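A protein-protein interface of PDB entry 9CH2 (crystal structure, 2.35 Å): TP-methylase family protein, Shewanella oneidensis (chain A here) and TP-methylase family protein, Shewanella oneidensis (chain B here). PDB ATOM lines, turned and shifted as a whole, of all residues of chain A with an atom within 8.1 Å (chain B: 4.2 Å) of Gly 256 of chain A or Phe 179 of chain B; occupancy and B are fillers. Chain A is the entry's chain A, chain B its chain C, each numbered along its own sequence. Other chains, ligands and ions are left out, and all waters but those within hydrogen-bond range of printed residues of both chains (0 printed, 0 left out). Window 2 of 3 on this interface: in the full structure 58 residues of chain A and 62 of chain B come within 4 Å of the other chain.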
ATOM      1  N   TYR A 249     -30.309  12.270  29.332  1.00  0.00           N
ATOM      2  CA  TYR A 249     -30.160  13.707  29.170  1.00  0.00           C
ATOM      3  C   TYR A 249     -29.655  14.327  30.472  1.00  0.00           C
ATOM      4  O   TYR A 249     -28.790  15.200  30.451  1.00  0.00           O
ATOM      5  CB  TYR A 249     -31.480  14.350  28.733  1.00  0.00           C
ATOM      6  CG  TYR A 249     -31.930  13.990  27.323  1.00  0.00           C
ATOM      7  CD1 TYR A 249     -31.323  14.560  26.210  1.00  0.00           C
ATOM      8  CD2 TYR A 249     -32.974  13.099  27.105  1.00  0.00           C
ATOM      9  CE1 TYR A 249     -31.729  14.243  24.924  1.00  0.00           C
ATOM     10  CE2 TYR A 249     -33.392  12.776  25.824  1.00  0.00           C
ATOM     11  CZ  TYR A 249     -32.767  13.350  24.731  1.00  0.00           C
ATOM     12  OH  TYR A 249     -33.174  13.033  23.467  1.00  0.00           O
ATOM     13  N   ALA A 250     -30.209  13.870  31.599  1.00  0.00           N
ATOM     14  CA  ALA A 250     -29.895  14.448  32.895  1.00  0.00           C
ATOM     15  C   ALA A 250     -28.397  14.341  33.173  1.00  0.00           C
ATOM     16  O   ALA A 250     -27.757  15.327  33.528  1.00  0.00           O
ATOM     17  CB  ALA A 250     -30.711  13.768  33.972  1.00  0.00           C
ATOM     18  N   ILE A 251     -27.848  13.132  33.010  1.00  0.00           N
ATOM     19  CA  ILE A 251     -26.449  12.882  33.317  1.00  0.00           C
ATOM     20  C   ILE A 251     -25.578  13.520  32.238  1.00  0.00           C
ATOM     21  O   ILE A 251     -24.541  14.106  32.541  1.00  0.00           O
ATOM     22  CB  ILE A 251     -26.177  11.373  33.462  1.00  0.00           C
ATOM     23  CG1 ILE A 251     -27.059  10.748  34.543  1.00  0.00           C
ATOM     24  CG2 ILE A 251     -24.694  11.105  33.720  1.00  0.00           C
ATOM     25  CD1 ILE A 251     -26.907  11.385  35.912  1.00  0.00           C
ATOM     26  N   LEU A 252     -26.011  13.399  30.979  1.00  0.00           N
ATOM     27  CA  LEU A 252     -25.312  14.022  29.868  1.00  0.00           C
ATOM     28  C   LEU A 252     -25.132  15.507  30.169  1.00  0.00           C
ATOM     29  O   LEU A 252     -24.052  16.060  29.976  1.00  0.00           O
ATOM     30  CB  LEU A 252     -26.085  13.805  28.568  1.00  0.00           C
ATOM     31  CG  LEU A 252     -26.089  12.374  28.020  1.00  0.00           C
ATOM     32  CD1 LEU A 252     -26.981  12.257  26.796  1.00  0.00           C
ATOM     33  CD2 LEU A 252     -24.677  11.920  27.696  1.00  0.00           C
ATOM     34  N   ALA A 253     -26.208  16.135  30.653  1.00  0.00           N
ATOM     35  CA  ALA A 253     -26.207  17.559  30.945  1.00  0.00           C
ATOM     36  C   ALA A 253     -25.071  17.892  31.908  1.00  0.00           C
ATOM     37  O   ALA A 253     -24.299  18.817  31.667  1.00  0.00           O
ATOM     38  CB  ALA A 253     -27.551  17.968  31.507  1.00  0.00           C
ATOM     39  N   LYS A 254     -24.976  17.123  32.997  1.00  0.00           N
ATOM     40  CA  LYS A 254     -23.989  17.382  34.033  1.00  0.00           C
ATOM     41  C   LYS A 254     -22.584  17.178  33.472  1.00  0.00           C
ATOM     42  O   LYS A 254     -21.638  17.825  33.916  1.00  0.00           O
ATOM     43  CB  LYS A 254     -24.251  16.505  35.265  1.00  0.00           C
ATOM     44  CG  LYS A 254     -25.432  16.950  36.120  1.00  0.00           C
ATOM     45  CD  LYS A 254     -25.539  16.246  37.469  1.00  0.00           C
ATOM     46  CE  LYS A 254     -26.012  14.832  37.359  1.00  0.00           C
ATOM     47  NZ  LYS A 254     -27.392  14.764  36.871  1.00  0.00           N
ATOM     48  N   LEU A 255     -22.458  16.277  32.492  1.00  0.00           N
ATOM     49  CA  LEU A 255     -21.174  16.005  31.867  1.00  0.00           C
ATOM     50  C   LEU A 255     -20.831  17.135  30.899  1.00  0.00           C
ATOM     51  O   LEU A 255     -19.660  17.368  30.603  1.00  0.00           O
ATOM     52  CB  LEU A 255     -21.206  14.647  31.166  1.00  0.00           C
ATOM     53  CG  LEU A 255     -21.217  13.421  32.085  1.00  0.00           C
ATOM     54  CD1 LEU A 255     -21.497  12.151  31.302  1.00  0.00           C
ATOM     55  CD2 LEU A 255     -19.905  13.303  32.841  1.00  0.00           C
ATOM     56  N   GLY A 256     -21.866  17.828  30.409  1.00  0.00           N
ATOM     57  CA  GLY A 256     -21.679  18.976  29.539  1.00  0.00           C
ATOM     58  C   GLY A 256     -22.275  18.741  28.153  1.00  0.00           C
ATOM     59  O   GLY A 256     -21.952  19.457  27.207  1.00  0.00           O
ATOM     60  N   ILE A 257     -23.150  17.736  28.047  1.00  0.00           N
ATOM     61  CA  ILE A 257     -23.798  17.409  26.787  1.00  0.00           C
ATOM     62  C   ILE A 257     -25.278  17.772  26.893  1.00  0.00           C
ATOM     63  O   ILE A 257     -26.021  17.142  27.641  1.00  0.00           O
ATOM     64  CB  ILE A 257     -23.610  15.922  26.437  1.00  0.00           C
ATOM     65  CG1 ILE A 257     -22.210  15.418  26.790  1.00  0.00           C
ATOM     66  CG2 ILE A 257     -23.948  15.664  24.968  1.00  0.00           C
ATOM     67  CD1 ILE A 257     -21.139  15.797  25.784  1.00  0.00           C
ATOM     68  N   GLY A 258     -25.691  18.792  26.132  1.00  0.00           N
ATOM     69  CA  GLY A 258     -27.079  19.225  26.111  1.00  0.00           C
ATOM     70  C   GLY A 258     -27.845  18.562  24.970  1.00  0.00           C
ATOM     71  O   GLY A 258     -27.253  17.899  24.122  1.00  0.00           O
ATOM     72  N   PRO A 259     -29.187  18.723  24.912  1.00  0.00           N
ATOM     73  CA  PRO A 259     -29.990  18.117  23.849  1.00  0.00           C
ATOM     74  C   PRO A 259     -29.624  18.677  22.478  1.00  0.00           C
ATOM     75  O   PRO A 259     -30.063  18.160  21.453  1.00  0.00           O
ATOM     76  CB  PRO A 259     -31.436  18.448  24.257  1.00  0.00           C
ATOM     77  CG  PRO A 259     -31.306  19.686  25.120  1.00  0.00           C
ATOM     78  CD  PRO A 259     -29.993  19.504  25.863  1.00  0.00           C
ATOM     79  N   ASP A 261     -26.641  18.651  21.618  1.00  0.00           N
ATOM     80  CA  ASP A 261     -25.468  17.846  21.322  1.00  0.00           C
ATOM     81  C   ASP A 261     -24.309  18.770  20.928  1.00  0.00           C
ATOM     82  O   ASP A 261     -23.655  19.294  21.859  1.00  0.00           O
ATOM     83  CB  ASP A 261     -25.767  16.814  20.245  1.00  0.00           C
ATOM     84  CG  ASP A 261     -26.948  15.897  20.531  1.00  0.00           C
ATOM     85  OD1 ASP A 261     -26.913  15.196  21.565  1.00  0.00           O
ATOM     86  OD2 ASP A 261     -27.895  15.888  19.716  1.00  0.00           O
ATOM     87  N   LEU B 176     -16.241  16.131  24.395  1.00  0.00           N
ATOM     88  CA  LEU B 176     -16.954  17.304  24.872  1.00  0.00           C
ATOM     89  C   LEU B 176     -17.065  17.284  26.396  1.00  0.00           C
ATOM     90  O   LEU B 176     -17.596  18.221  26.987  1.00  0.00           O
ATOM     91  CB  LEU B 176     -18.333  17.356  24.216  1.00  0.00           C
ATOM     92  CG  LEU B 176     -18.350  17.456  22.687  1.00  0.00           C
ATOM     93  CD1 LEU B 176     -19.773  17.393  22.156  1.00  0.00           C
ATOM     94  CD2 LEU B 176     -17.662  18.723  22.210  1.00  0.00           C
ATOM     95  N   THR B 177     -16.559  16.218  27.027  1.00  0.00           N
ATOM     96  CA  THR B 177     -16.668  16.069  28.470  1.00  0.00           C
ATOM     97  C   THR B 177     -15.279  16.126  29.099  1.00  0.00           C
ATOM     98  O   THR B 177     -15.131  15.908  30.299  1.00  0.00           O
ATOM     99  CB  THR B 177     -17.367  14.752  28.809  1.00  0.00           C
ATOM    100  OG1 THR B 177     -16.407  13.729  28.566  1.00  0.00           O
ATOM    101  CG2 THR B 177     -18.617  14.519  27.981  1.00  0.00           C
ATOM    102  N   GLN B 178     -14.265  16.427  28.280  1.00  0.00           N
ATOM    103  CA  GLN B 178     -12.881  16.322  28.709  1.00  0.00           C
ATOM    104  C   GLN B 178     -12.432  17.620  29.376  1.00  0.00           C
ATOM    105  O   GLN B 178     -11.313  17.705  29.876  1.00  0.00           O
ATOM    106  CB  GLN B 178     -11.996  15.925  27.527  1.00  0.00           C
ATOM    107  CG  GLN B 178     -12.119  14.453  27.147  1.00  0.00           C
ATOM    108  CD  GLN B 178     -11.471  14.116  25.822  1.00  0.00           C
ATOM    109  OE1 GLN B 178     -10.890  14.975  25.149  1.00  0.00           O
ATOM    110  NE2 GLN B 178     -11.568  12.853  25.433  1.00  0.00           N
ATOM    111  N   PHE B 179     -13.314  18.626  29.383  1.00  0.00           N
ATOM    112  CA  PHE B 179     -13.086  19.825  30.169  1.00  0.00           C
ATOM    113  C   PHE B 179     -13.257  19.456  31.640  1.00  0.00           C
ATOM    114  O   PHE B 179     -12.842  20.196  32.530  1.00  0.00           O
ATOM    115  CB  PHE B 179     -14.035  20.947  29.733  1.00  0.00           C
ATOM    116  CG  PHE B 179     -15.496  20.716  30.093  1.00  0.00           C
ATOM    117  CD1 PHE B 179     -16.289  19.856  29.342  1.00  0.00           C
ATOM    118  CD2 PHE B 179     -16.076  21.368  31.176  1.00  0.00           C
ATOM    119  CE1 PHE B 179     -17.618  19.647  29.672  1.00  0.00           C
ATOM    120  CE2 PHE B 179     -17.408  21.158  31.499  1.00  0.00           C
ATOM    121  CZ  PHE B 179     -18.175  20.299  30.747  1.00  0.00           C
ATOM    122  N   HIS B 180     -13.877  18.293  31.870  1.00  0.00           N
ATOM    123  CA  HIS B 180     -14.044  17.746  33.206  1.00  0.00           C
ATOM    124  C   HIS B 180     -12.842  16.873  33.553  1.00  0.00           C
ATOM    125  O   HIS B 180     -12.139  16.390  32.668  1.00  0.00           O
ATOM    126  CB  HIS B 180     -15.345  16.941  33.305  1.00  0.00           C
ATOM    127  CG  HIS B 180     -16.564  17.766  33.558  1.00  0.00           C
ATOM    128  ND1 HIS B 180     -16.551  18.891  34.354  1.00  0.00           N
ATOM    129  CD2 HIS B 180     -17.829  17.622  33.142  1.00  0.00           C
ATOM    130  CE1 HIS B 180     -17.771  19.406  34.401  1.00  0.00           C
ATOM    131  NE2 HIS B 180     -18.563  18.652  33.672  1.00  0.00           N
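Of the printed residues of chain B, Gly 256 of chain A touches Phe 179 (3.9 Å). Of the printed residues of chain B, Lys 254 of chain A touches His 180 (3.2 Å). Printed residues of chain A within 4 Å of His 180 of chain B: Lys 254 and Leu 255. Of the printed residues of chain B, Ile 257 of chain A touches Leu 176 and Thr 177. Printed residues of chain A within 4 Å of Thr 177 of chain B: Leu 255 and Ile 257. Printed residues of chain A within 4 Å of Leu 176 of chain B: Ile 257. Gly 258 of chain A touches none of the printed residues of chain B. Ala 253 of chain A touches none of the printed residues of chain B. The nearest printed residue of chain A that does not touch Leu 176 of chain B is Leu 255 of chain A (4.3 Å).
Printed residues of chain A that touch a printed residue of chain B: Lys 254, Leu 255, Gly 256 and Ile 257. Hydrophobic or aromatic side chains of chain A within 4 Å of the printed part of chain B: Ile 257. Of the 5 printed residues of chain B, 4 touch a printed residue of chain A. Printed residues of chain B that touch a printed residue of chain A: Leu 176, Thr 177, Phe 179 and His 180. Among the printed residues, 7 pairs touch across the chains. Among the printed residues, no Asp or Glu carboxylate lies within 4 Å of a Lys or Arg side-chain nitrogen of the other chain.
The backbone carbonyl oxygen of Ala 250 of chain A is in hydrogen-bond range of the side-chain amino group of Lys 254 of chain A. The backbone carbonyl oxygen (O) of Leu 252 of chain A lies within hydrogen-bond range of the backbone NH (N) of Ile 257 of chain A.
O of Lys 254 of chain A lies within hydrogen-bond range of NE2 of His 180 of chain B, 3.2 Å away.
Thr 177 of chain B touches Leu 255 of chain A. Leu 255 of chain A touches Phe 179 of chain B (O to CE1, 3.2 Å). Leu 255 of chain A touches His 180 of chain B. Phe 179 of chain B touches Gly 256 of chain A (CZ to CA, 3.9 Å). Leu 176 of chain B touches Ile 257 of chain A (CB to CD1, 3.6 Å). CD1 of Ile 257 of chain A touches CG2 of Thr 177 of chain B, 3.6 Å away.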
